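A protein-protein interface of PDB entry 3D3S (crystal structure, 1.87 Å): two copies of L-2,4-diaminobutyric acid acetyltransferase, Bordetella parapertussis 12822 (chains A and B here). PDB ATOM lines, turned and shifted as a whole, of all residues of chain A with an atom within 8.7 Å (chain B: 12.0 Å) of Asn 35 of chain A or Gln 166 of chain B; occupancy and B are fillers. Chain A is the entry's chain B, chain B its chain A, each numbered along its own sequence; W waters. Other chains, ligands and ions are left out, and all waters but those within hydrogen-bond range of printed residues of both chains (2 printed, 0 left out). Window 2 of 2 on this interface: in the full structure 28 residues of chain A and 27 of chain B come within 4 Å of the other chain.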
ATOM      1  N   ARG A  30      15.712  13.316 -23.385  1.00  0.00           N
ATOM      2  CA  ARG A  30      16.759  13.897 -24.188  1.00  0.00           C
ATOM      3  C   ARG A  30      17.002  15.323 -23.693  1.00  0.00           C
ATOM      4  O   ARG A  30      16.104  15.944 -23.015  1.00  0.00           O
ATOM      5  CB  ARG A  30      16.319  13.929 -25.660  1.00  0.00           C
ATOM      6  CG  ARG A  30      15.083  14.771 -25.889  1.00  0.00           C
ATOM      7  CD  ARG A  30      14.763  14.885 -27.340  1.00  0.00           C
ATOM      8  NE  ARG A  30      13.540  15.644 -27.600  1.00  0.00           N
ATOM      9  CZ  ARG A  30      13.420  16.976 -27.547  1.00  0.00           C
ATOM     10  NH1 ARG A  30      14.422  17.754 -27.158  1.00  0.00           N
ATOM     11  NH2 ARG A  30      12.257  17.539 -27.845  1.00  0.00           N
ATOM     12  N   PRO A  32      16.988  19.316 -23.792  1.00  0.00           N
ATOM     13  CA  PRO A  32      16.116  20.231 -24.483  1.00  0.00           C
ATOM     14  C   PRO A  32      16.858  20.981 -25.614  1.00  0.00           C
ATOM     15  O   PRO A  32      18.087  21.073 -25.594  1.00  0.00           O
ATOM     16  CB  PRO A  32      15.655  21.164 -23.368  1.00  0.00           C
ATOM     17  CG  PRO A  32      16.878  21.293 -22.479  1.00  0.00           C
ATOM     18  CD  PRO A  32      17.365  19.825 -22.449  1.00  0.00           C
ATOM     19  N   ARG A  33      16.104  21.480 -26.585  1.00  0.00           N
ATOM     20  CA  ARG A  33      16.600  22.295 -27.682  1.00  0.00           C
ATOM     21  C   ARG A  33      15.753  23.554 -27.737  1.00  0.00           C
ATOM     22  O   ARG A  33      14.649  23.587 -27.175  1.00  0.00           O
ATOM     23  CB  ARG A  33      16.445  21.520 -29.021  1.00  0.00           C
ATOM     24  CG  ARG A  33      17.099  20.140 -29.028  1.00  0.00           C
ATOM     25  CD  ARG A  33      16.888  19.400 -30.393  1.00  0.00           C
ATOM     26  NE  ARG A  33      15.477  19.080 -30.648  1.00  0.00           N
ATOM     27  CZ  ARG A  33      14.977  17.844 -30.657  1.00  0.00           C
ATOM     28  NH1 ARG A  33      15.781  16.807 -30.451  1.00  0.00           N
ATOM     29  NH2 ARG A  33      13.677  17.631 -30.905  1.00  0.00           N
ATOM     30  N   ARG A  34      16.250  24.581 -28.423  1.00  0.00           N
ATOM     31  CA  ARG A  34      15.585  25.896 -28.470  1.00  0.00           C
ATOM     32  C   ARG A  34      14.078  25.802 -28.763  1.00  0.00           C
ATOM     33  O   ARG A  34      13.264  26.485 -28.093  1.00  0.00           O
ATOM     34  CB  ARG A  34      16.280  26.803 -29.485  1.00  0.00           C
ATOM     35  CG  ARG A  34      15.842  28.219 -29.401  1.00  0.00           C
ATOM     36  CD  ARG A  34      16.566  29.035 -30.438  1.00  0.00           C
ATOM     37  NE  ARG A  34      18.005  29.051 -30.220  1.00  0.00           N
ATOM     38  CZ  ARG A  34      18.856  29.597 -31.070  1.00  0.00           C
ATOM     39  NH1 ARG A  34      20.162  29.559 -30.801  1.00  0.00           N
ATOM     40  NH2 ARG A  34      18.402  30.162 -32.211  1.00  0.00           N
ATOM     41  N   ASN A  35      13.700  24.919 -29.707  1.00  0.00           N
ATOM     42  CA  ASN A  35      12.302  24.811 -30.086  1.00  0.00           C
ATOM     43  C   ASN A  35      11.434  24.149 -29.038  1.00  0.00           C
ATOM     44  O   ASN A  35      10.199  24.065 -29.232  1.00  0.00           O
ATOM     45  CB  ASN A  35      12.119  24.122 -31.471  1.00  0.00           C
ATOM     46  CG  ASN A  35      11.838  25.141 -32.595  1.00  0.00           C
ATOM     47  OD1 ASN A  35      11.535  26.313 -32.322  1.00  0.00           O
ATOM     48  ND2 ASN A  35      12.010  24.716 -33.867  1.00  0.00           N
ATOM     49  N   ASP A  36      12.054  23.669 -27.953  1.00  0.00           N
ATOM     50  CA  ASP A  36      11.308  23.124 -26.826  1.00  0.00           C
ATOM     51  C   ASP A  36      10.924  24.214 -25.793  1.00  0.00           C
ATOM     52  O   ASP A  36      10.098  23.937 -24.906  1.00  0.00           O
ATOM     53  CB  ASP A  36      12.153  22.122 -26.042  1.00  0.00           C
ATOM     54  CG  ASP A  36      12.460  20.859 -26.810  1.00  0.00           C
ATOM     55  OD1 ASP A  36      11.654  20.366 -27.637  1.00  0.00           O
ATOM     56  OD2 ASP A  36      13.526  20.315 -26.518  1.00  0.00           O
ATOM     57  N   GLY A  37      11.574  25.389 -25.847  1.00  0.00           N
ATOM     58  CA  GLY A  37      11.443  26.400 -24.754  1.00  0.00           C
ATOM     59  C   GLY A  37      10.005  26.808 -24.475  1.00  0.00           C
ATOM     60  O   GLY A  37       9.612  26.888 -23.298  1.00  0.00           O
ATOM     61  N   ALA A  38       9.221  27.073 -25.539  1.00  0.00           N
ATOM     62  CA  ALA A  38       7.804  27.481 -25.401  1.00  0.00           C
ATOM     63  C   ALA A  38       7.026  26.365 -24.728  1.00  0.00           C
ATOM     64  O   ALA A  38       6.237  26.608 -23.806  1.00  0.00           O
ATOM     65  CB  ALA A  38       7.174  27.825 -26.710  1.00  0.00           C
ATOM     66  N   ALA A  39       7.326  25.140 -25.116  1.00  0.00           N
ATOM     67  CA  ALA A  39       6.584  24.001 -24.572  1.00  0.00           C
ATOM     68  C   ALA A  39       6.952  23.715 -23.139  1.00  0.00           C
ATOM     69  O   ALA A  39       6.102  23.266 -22.353  1.00  0.00           O
ATOM     70  CB  ALA A  39       6.780  22.736 -25.489  1.00  0.00           C
ATOM     71  N   ILE A  40       8.219  23.896 -22.778  1.00  0.00           N
ATOM     72  CA  ILE A  40       8.652  23.722 -21.386  1.00  0.00           C
ATOM     73  C   ILE A  40       8.005  24.778 -20.497  1.00  0.00           C
ATOM     74  O   ILE A  40       7.571  24.463 -19.415  1.00  0.00           O
ATOM     75  CB  ILE A  40      10.210  23.889 -21.310  1.00  0.00           C
ATOM     76  CG1 ILE A  40      10.893  22.680 -22.051  1.00  0.00           C
ATOM     77  CG2 ILE A  40      10.721  24.122 -19.798  1.00  0.00           C
ATOM     78  CD1 ILE A  40      12.470  22.960 -22.335  1.00  0.00           C
ATOM     79  N   LEU A  55       9.311  33.115 -20.144  1.00  0.00           N
ATOM     80  CA  LEU A  55       9.692  32.277 -21.270  1.00  0.00           C
ATOM     81  C   LEU A  55      11.173  32.376 -21.647  1.00  0.00           C
ATOM     82  O   LEU A  55      11.778  31.345 -21.891  1.00  0.00           O
ATOM     83  CB  LEU A  55       8.797  32.607 -22.456  1.00  0.00           C
ATOM     84  CG  LEU A  55       8.885  31.798 -23.792  1.00  0.00           C
ATOM     85  CD1 LEU A  55       9.462  30.468 -23.690  1.00  0.00           C
ATOM     86  CD2 LEU A  55       7.462  31.747 -24.386  1.00  0.00           C
ATOM     87  N   TYR A  58      13.421  30.073 -19.624  1.00  0.00           N
ATOM     88  CA  TYR A  58      13.427  28.716 -20.144  1.00  0.00           C
ATOM     89  C   TYR A  58      14.256  28.578 -21.431  1.00  0.00           C
ATOM     90  O   TYR A  58      14.982  27.585 -21.610  1.00  0.00           O
ATOM     91  CB  TYR A  58      12.000  28.141 -20.274  1.00  0.00           C
ATOM     92  CG  TYR A  58      11.360  28.054 -18.877  1.00  0.00           C
ATOM     93  CD1 TYR A  58      11.793  27.083 -17.949  1.00  0.00           C
ATOM     94  CD2 TYR A  58      10.430  28.982 -18.501  1.00  0.00           C
ATOM     95  CE1 TYR A  58      11.277  27.032 -16.610  1.00  0.00           C
ATOM     96  CE2 TYR A  58       9.940  28.995 -17.185  1.00  0.00           C
ATOM     97  CZ  TYR A  58      10.368  27.999 -16.256  1.00  0.00           C
ATOM     98  OH  TYR A  58       9.869  28.091 -14.977  1.00  0.00           O
ATOM     99  N   LEU A  59      14.160  29.563 -22.312  1.00  0.00           N
ATOM    100  CA  LEU A  59      15.014  29.539 -23.515  1.00  0.00           C
ATOM    101  C   LEU A  59      16.514  29.553 -23.174  1.00  0.00           C
ATOM    102  O   LEU A  59      17.308  28.851 -23.795  1.00  0.00           O
ATOM    103  CB  LEU A  59      14.650  30.711 -24.422  1.00  0.00           C
ATOM    104  CG  LEU A  59      13.302  30.497 -25.153  1.00  0.00           C
ATOM    105  CD1 LEU A  59      13.091  31.886 -25.813  1.00  0.00           C
ATOM    106  CD2 LEU A  59      13.406  29.408 -26.239  1.00  0.00           C
ATOM    107  N   CYS A  62      17.554  26.138 -22.305  1.00  0.00           N
ATOM    108  CA  CYS A  62      17.792  25.350 -23.515  1.00  0.00           C
ATOM    109  C   CYS A  62      19.100  25.709 -24.193  1.00  0.00           C
ATOM    110  O   CYS A  62      19.802  24.808 -24.742  1.00  0.00           O
ATOM    111  CB  CYS A  62      16.625  25.561 -24.524  1.00  0.00           C
ATOM    112  SG  CYS A  62      14.999  25.063 -23.963  1.00  0.00           S
ATOM    113  N   GLU A  63      19.435  27.006 -24.228  1.00  0.00           N
ATOM    114  CA  GLU A  63      20.615  27.456 -24.920  1.00  0.00           C
ATOM    115  C   GLU A  63      21.942  27.190 -24.200  1.00  0.00           C
ATOM    116  O   GLU A  63      22.958  26.864 -24.824  1.00  0.00           O
ATOM    117  CB  GLU A  63      20.570  28.944 -25.147  1.00  0.00           C
ATOM    118  CG  GLU A  63      19.616  29.389 -26.156  1.00  0.00           C
ATOM    119  CD  GLU A  63      19.877  28.765 -27.507  1.00  0.00           C
ATOM    120  OE1 GLU A  63      18.931  28.107 -27.951  1.00  0.00           O
ATOM    121  OE2 GLU A  63      20.977  28.928 -28.099  1.00  0.00           O
ATOM    122  N   VAL A  71      14.207  16.827 -21.076  1.00  0.00           N
ATOM    123  CA  VAL A  71      12.766  16.791 -21.349  1.00  0.00           C
ATOM    124  C   VAL A  71      12.357  15.354 -21.567  1.00  0.00           C
ATOM    125  O   VAL A  71      13.166  14.492 -21.983  1.00  0.00           O
ATOM    126  CB  VAL A  71      12.305  17.701 -22.586  1.00  0.00           C
ATOM    127  CG1 VAL A  71      12.580  19.190 -22.297  1.00  0.00           C
ATOM    128  CG2 VAL A  71      13.056  17.292 -23.840  1.00  0.00           C
ATOM    129  N   GLY A  77       5.026  13.613 -29.366  1.00  0.00           N
ATOM    130  CA  GLY A  77       5.859  14.820 -29.349  1.00  0.00           C
ATOM    131  C   GLY A  77       5.518  15.829 -28.261  1.00  0.00           C
ATOM    132  O   GLY A  77       5.985  16.961 -28.276  1.00  0.00           O
ATOM    133  N   ILE A  79       5.732  17.478 -24.604  1.00  0.00           N
ATOM    134  CA  ILE A  79       6.711  17.476 -23.517  1.00  0.00           C
ATOM    135  C   ILE A  79       5.969  17.431 -22.209  1.00  0.00           C
ATOM    136  O   ILE A  79       5.285  18.406 -21.831  1.00  0.00           O
ATOM    137  CB  ILE A  79       7.656  18.667 -23.621  1.00  0.00           C
ATOM    138  CG1 ILE A  79       8.560  18.392 -24.856  1.00  0.00           C
ATOM    139  CG2 ILE A  79       8.419  18.764 -22.339  1.00  0.00           C
ATOM    140  CD1 ILE A  79       8.968  19.586 -25.465  1.00  0.00           C
ATOM    141  N   PRO B 161      20.194  37.518 -35.896  1.00  0.00           N
ATOM    142  CA  PRO B 161      18.921  37.005 -35.407  1.00  0.00           C
ATOM    143  C   PRO B 161      19.143  35.795 -34.475  1.00  0.00           C
ATOM    144  O   PRO B 161      20.081  35.013 -34.691  1.00  0.00           O
ATOM    145  CB  PRO B 161      18.227  36.506 -36.672  1.00  0.00           C
ATOM    146  CG  PRO B 161      19.216  36.729 -37.771  1.00  0.00           C
ATOM    147  CD  PRO B 161      20.220  37.669 -37.355  1.00  0.00           C
ATOM    148  N   PHE B 162      18.274  35.633 -33.491  1.00  0.00           N
ATOM    149  CA  PHE B 162      18.494  34.613 -32.465  1.00  0.00           C
ATOM    150  C   PHE B 162      17.163  34.060 -31.956  1.00  0.00           C
ATOM    151  O   PHE B 162      16.781  32.936 -32.349  1.00  0.00           O
ATOM    152  CB  PHE B 162      19.345  35.262 -31.402  1.00  0.00           C
ATOM    153  CG  PHE B 162      19.820  34.365 -30.312  1.00  0.00           C
ATOM    154  CD1 PHE B 162      20.576  33.204 -30.572  1.00  0.00           C
ATOM    155  CD2 PHE B 162      19.589  34.754 -28.983  1.00  0.00           C
ATOM    156  CE1 PHE B 162      21.062  32.408 -29.494  1.00  0.00           C
ATOM    157  CE2 PHE B 162      20.088  33.980 -27.908  1.00  0.00           C
ATOM    158  CZ  PHE B 162      20.783  32.795 -28.149  1.00  0.00           C
ATOM    159  N   PHE B 163      16.457  34.783 -31.076  1.00  0.00           N
ATOM    160  CA  PHE B 163      15.148  34.321 -30.664  1.00  0.00           C
ATOM    161  C   PHE B 163      14.125  35.076 -31.448  1.00  0.00           C
ATOM    162  O   PHE B 163      14.075  36.309 -31.341  1.00  0.00           O
ATOM    163  CB  PHE B 163      14.879  34.575 -29.180  1.00  0.00           C
ATOM    164  CG  PHE B 163      15.772  33.796 -28.223  1.00  0.00           C
ATOM    165  CD1 PHE B 163      16.352  32.590 -28.595  1.00  0.00           C
ATOM    166  CD2 PHE B 163      15.968  34.263 -26.916  1.00  0.00           C
ATOM    167  CE1 PHE B 163      17.160  31.849 -27.653  1.00  0.00           C
ATOM    168  CE2 PHE B 163      16.750  33.554 -25.974  1.00  0.00           C
ATOM    169  CZ  PHE B 163      17.332  32.319 -26.345  1.00  0.00           C
ATOM    170  N   ASP B 164      13.294  34.363 -32.193  1.00  0.00           N
ATOM    171  CA  ASP B 164      12.296  35.016 -33.017  1.00  0.00           C
ATOM    172  C   ASP B 164      10.922  34.541 -32.551  1.00  0.00           C
ATOM    173  O   ASP B 164      10.826  33.913 -31.502  1.00  0.00           O
ATOM    174  CB  ASP B 164      12.553  34.627 -34.466  1.00  0.00           C
ATOM    175  CG  ASP B 164      12.559  33.122 -34.685  1.00  0.00           C
ATOM    176  OD1 ASP B 164      12.594  32.305 -33.705  1.00  0.00           O
ATOM    177  OD2 ASP B 164      12.560  32.740 -35.864  1.00  0.00           O
ATOM    178  N   ARG B 165       9.889  34.760 -33.363  1.00  0.00           N
ATOM    179  CA  ARG B 165       8.552  34.213 -33.110  1.00  0.00           C
ATOM    180  C   ARG B 165       8.516  32.692 -32.887  1.00  0.00           C
ATOM    181  O   ARG B 165       7.755  32.201 -32.053  1.00  0.00           O
ATOM    182  CB  ARG B 165       7.592  34.563 -34.258  1.00  0.00           C
ATOM    183  CG  ARG B 165       7.304  36.059 -34.369  1.00  0.00           C
ATOM    184  CD  ARG B 165       6.593  36.406 -35.680  1.00  0.00           C
ATOM    185  NE  ARG B 165       6.735  37.823 -36.013  1.00  0.00           N
ATOM    186  CZ  ARG B 165       6.009  38.808 -35.480  1.00  0.00           C
ATOM    187  NH1 ARG B 165       5.072  38.546 -34.573  1.00  0.00           N
ATOM    188  NH2 ARG B 165       6.213  40.067 -35.857  1.00  0.00           N
ATOM    189  N   GLN B 166       9.320  31.953 -33.649  1.00  0.00           N
ATOM    190  CA  GLN B 166       9.388  30.503 -33.523  1.00  0.00           C
ATOM    191  C   GLN B 166       9.826  30.111 -32.103  1.00  0.00           C
ATOM    192  O   GLN B 166       9.235  29.233 -31.469  1.00  0.00           O
ATOM    193  CB  GLN B 166      10.351  29.921 -34.588  1.00  0.00           C
ATOM    194  CG  GLN B 166      10.273  28.387 -34.789  1.00  0.00           C
ATOM    195  CD  GLN B 166      11.178  27.864 -35.907  1.00  0.00           C
ATOM    196  OE1 GLN B 166      11.819  28.639 -36.606  1.00  0.00           O
ATOM    197  NE2 GLN B 166      11.212  26.534 -36.091  1.00  0.00           N
ATOM    198  N   ALA B 167      10.857  30.797 -31.613  1.00  0.00           N
ATOM    199  CA  ALA B 167      11.459  30.482 -30.330  1.00  0.00           C
ATOM    200  C   ALA B 167      10.511  30.835 -29.162  1.00  0.00           C
ATOM    201  O   ALA B 167      10.491  30.107 -28.142  1.00  0.00           O
ATOM    202  CB  ALA B 167      12.778  31.210 -30.161  1.00  0.00           C
ATOM    203  N   PHE B 168       9.703  31.894 -29.337  1.00  0.00           N
ATOM    204  CA  PHE B 168       8.704  32.288 -28.301  1.00  0.00           C
ATOM    205  C   PHE B 168       7.356  31.630 -28.411  1.00  0.00           C
ATOM    206  O   PHE B 168       6.459  31.928 -27.604  1.00  0.00           O
ATOM    207  CB  PHE B 168       8.538  33.819 -28.219  1.00  0.00           C
ATOM    208  CG  PHE B 168       9.748  34.542 -27.695  1.00  0.00           C
ATOM    209  CD1 PHE B 168       9.999  34.594 -26.295  1.00  0.00           C
ATOM    210  CD2 PHE B 168      10.607  35.238 -28.557  1.00  0.00           C
ATOM    211  CE1 PHE B 168      11.103  35.301 -25.753  1.00  0.00           C
ATOM    212  CE2 PHE B 168      11.722  35.894 -28.063  1.00  0.00           C
ATOM    213  CZ  PHE B 168      11.990  35.972 -26.656  1.00  0.00           C
ATOM    214  N   GLY B 169       7.201  30.765 -29.394  1.00  0.00           N
ATOM    215  CA  GLY B 169       5.932  30.050 -29.611  1.00  0.00           C
ATOM    216  C   GLY B 169       4.773  30.988 -29.878  1.00  0.00           C
ATOM    217  O   GLY B 169       3.619  30.678 -29.554  1.00  0.00           O
ATOM    218  N   GLY B 170       5.049  32.129 -30.498  1.00  0.00           N
ATOM    219  CA  GLY B 170       3.971  33.065 -30.819  1.00  0.00           C
ATOM    220  C   GLY B 170       3.558  33.922 -29.634  1.00  0.00           C
ATOM    221  O   GLY B 170       2.564  34.622 -29.701  1.00  0.00           O
ATOM    222  N   ALA B 171       4.335  33.931 -28.549  1.00  0.00           N
ATOM    223  CA  ALA B 171       3.916  34.680 -27.380  1.00  0.00           C
ATOM    224  C   ALA B 171       4.107  36.150 -27.683  1.00  0.00           C
ATOM    225  O   ALA B 171       4.825  36.503 -28.601  1.00  0.00           O
ATOM    226  CB  ALA B 171       4.739  34.265 -26.156  1.00  0.00           C
ATOM    227  N   ASP B 172       3.441  37.006 -26.930  1.00  0.00           N
ATOM    228  CA  ASP B 172       3.556  38.439 -27.136  1.00  0.00           C
ATOM    229  C   ASP B 172       4.870  38.949 -26.520  1.00  0.00           C
ATOM    230  O   ASP B 172       4.898  39.500 -25.408  1.00  0.00           O
ATOM    231  CB  ASP B 172       2.317  39.097 -26.514  1.00  0.00           C
ATOM    232  CG  ASP B 172       2.156  40.547 -26.884  1.00  0.00           C
ATOM    233  OD1 ASP B 172       3.066  41.159 -27.512  1.00  0.00           O
ATOM    234  OD2 ASP B 172       1.085  41.085 -26.511  1.00  0.00           O
ATOM    235  N   HIS B 173       5.966  38.744 -27.244  1.00  0.00           N
ATOM    236  CA  HIS B 173       7.304  39.172 -26.799  1.00  0.00           C
ATOM    237  C   HIS B 173       8.072  39.614 -28.048  1.00  0.00           C
ATOM    238  O   HIS B 173       7.985  38.991 -29.086  1.00  0.00           O
ATOM    239  CB  HIS B 173       8.001  37.999 -26.075  1.00  0.00           C
ATOM    240  CG  HIS B 173       9.251  38.378 -25.326  1.00  0.00           C
ATOM    241  ND1 HIS B 173      10.385  38.827 -25.958  1.00  0.00           N
ATOM    242  CD2 HIS B 173       9.559  38.339 -23.998  1.00  0.00           C
ATOM    243  CE1 HIS B 173      11.339  39.065 -25.072  1.00  0.00           C
ATOM    244  NE2 HIS B 173      10.865  38.767 -23.870  1.00  0.00           N
ATOM    245  N   ASP B 174       8.801  40.725 -27.966  1.00  0.00           N
ATOM    246  CA  ASP B 174       9.633  41.134 -29.092  1.00  0.00           C
ATOM    247  C   ASP B 174      10.688  40.048 -29.362  1.00  0.00           C
ATOM    248  O   ASP B 174      11.061  39.285 -28.423  1.00  0.00           O
ATOM    249  CB  ASP B 174      10.385  42.407 -28.713  1.00  0.00           C
ATOM    250  CG  ASP B 174       9.475  43.636 -28.650  1.00  0.00           C
ATOM    251  OD1 ASP B 174       8.344  43.592 -29.202  1.00  0.00           O
ATOM    252  OD2 ASP B 174       9.908  44.642 -28.038  1.00  0.00           O
ATOM    253  N   ASP B 175      11.178  40.010 -30.607  1.00  0.00           N
ATOM    254  CA  ASP B 175      12.344  39.219 -30.979  1.00  0.00           C
ATOM    255  C   ASP B 175      13.542  39.666 -30.140  1.00  0.00           C
ATOM    256  O   ASP B 175      13.603  40.828 -29.766  1.00  0.00           O
ATOM    257  CB  ASP B 175      12.663  39.507 -32.444  1.00  0.00           C
ATOM    258  CG  ASP B 175      11.733  38.788 -33.411  1.00  0.00           C
ATOM    259  OD1 ASP B 175      10.813  38.050 -32.964  1.00  0.00           O
ATOM    260  OD2 ASP B 175      11.925  38.960 -34.643  1.00  0.00           O
ATOM    261  N   GLU B 176      14.481  38.760 -29.855  1.00  0.00           N
ATOM    262  CA  GLU B 176      15.717  39.100 -29.167  1.00  0.00           C
ATOM    263  C   GLU B 176      16.888  38.700 -30.048  1.00  0.00           C
ATOM    264  O   GLU B 176      17.104  37.490 -30.252  1.00  0.00           O
ATOM    265  CB  GLU B 176      15.796  38.333 -27.856  1.00  0.00           C
ATOM    266  CG  GLU B 176      14.699  38.723 -26.854  1.00  0.00           C
ATOM    267  CD  GLU B 176      15.100  39.915 -25.978  1.00  0.00           C
ATOM    268  OE1 GLU B 176      16.323  40.267 -25.798  1.00  0.00           O
ATOM    269  OE2 GLU B 176      14.147  40.530 -25.440  1.00  0.00           O
ATOM    270  N   MET B 177      17.633  39.686 -30.567  1.00  0.00           N
ATOM    271  CA  MET B 177      18.803  39.381 -31.365  1.00  0.00           C
ATOM    272  C   MET B 177      20.042  39.106 -30.488  1.00  0.00           C
ATOM    273  O   MET B 177      20.126  39.636 -29.391  1.00  0.00           O
ATOM    274  CB  MET B 177      19.066  40.536 -32.326  1.00  0.00           C
ATOM    275  CG  MET B 177      17.981  40.456 -33.500  1.00  0.00           C
ATOM    276  SD  MET B 177      16.367  41.349 -32.858  1.00  0.00           S
ATOM    277  CE  MET B 177      17.104  43.124 -32.751  1.00  0.00           C
HETATM  278  O   HOH W   1       8.796  26.839 -30.275  1.00  0.00           O
HETATM  279  O   HOH W   2      10.544  27.475 -28.118  1.00  0.00           O
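Water W2 lies within hydrogen-bond range of O of Ala 167 of chain B (2.6 Å), O of Arg 34 of chain A (2.9 Å), N of Ala 38 of chain A (2.9 Å) and N of Gly 37 of chain A (3.3 Å).
Water W1 lies within hydrogen-bond range of O of Gln 166 of chain B and O of Asn 35 of chain A.
Of the 18 printed residues of chain A, 6 touch a printed residue of chain B.
Hydrophobic or aromatic side chains of chain A that line the printed part of chain B: Ala 38, Leu 55 and Leu 59.
Among the printed residues, 10 pairs touch across the chains.
No position is printed for both chains.
N of Glu 176 of chain B is in hydrogen-bond range of O of Phe 163 of chain B, 2.9 Å away.
The backbone NH of Gln 166 of chain B lies close to the side-chain carboxylate of Asp 164 of chain B, at 3.3 Å.
The side-chain carboxylate of Asp 164 of chain B sits at hydrogen-bond distance from the backbone NH of Ala 167 of chain B, at 3.1 Å.
The side-chain carboxylate (OE1) of Glu 63 of chain A lies within salt-bridge range of the guanidinium group (NE) of Arg 34 of chain A (2.6 Å).
The backbone carbonyl oxygen (O) of Phe 162 of chain B sits at hydrogen-bond distance from the guanidinium group (NH2) of Arg 34 of chain A, 3.2 Å away.
NE2 of Gln 166 of chain B lies close to ND2 of Asn 35 of chain A (3.0 Å).
Of the printed residues of chain B, Asn 35 of chain A touches Gln 166.
Printed residues of chain A within 4 Å of Gln 166 of chain B: Asn 35 (3.0 Å).
Asp 36 of chain A touches none of the printed residues of chain B.
Gly 37 of chain A touches none of the printed residues of chain B.
Of chain B, only Gly 169 (3.9 Å) comes within 4 Å of Ala 38 of chain A.
Of chain A, only Leu 59 comes within 4 Å of Ala 167 of chain B.
Printed residues of chain A within 4 Å of Phe 163 of chain B: Arg 34 (3.9 Å), Leu 59 (3.7 Å) and Glu 63 (3.7 Å).
Printed residues of chain A within 4 Å of Gly 169 of chain B: Ala 38 (3.9 Å).
Printed residues of chain B within 4 Å of Arg 34 of chain A: Phe 162 and Phe 163.
Printed residues of chain B within 4 Å of Glu 63 of chain A: Phe 162 and Phe 163.
Printed residues of chain A within 4 Å of Phe 162 of chain B: Arg 34 (3.2 Å) and Glu 63 (3.8 Å).
The nearest printed residue of chain B that does not touch Asn 35 of chain A is Ala 167 of chain B (4.6 Å).
Arg 34 of chain A touches Phe 163 of chain B.
Ala 38 of chain A touches Gly 169 of chain B.
Leu 55 of chain A touches Phe 168 of chain B.
Phe 163 of chain B touches Leu 59 of chain A.
CD2 of Leu 59 of chain A touches O of Ala 167 of chain B (3.6 Å).
Leu 59 of chain A touches Phe 168 of chain B (CD1 to CE1, 3.95 Å).
Glu 63 of chain A touches Phe 162 of chain B.
Phe 163 of chain B touches Glu 63 of chain A.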
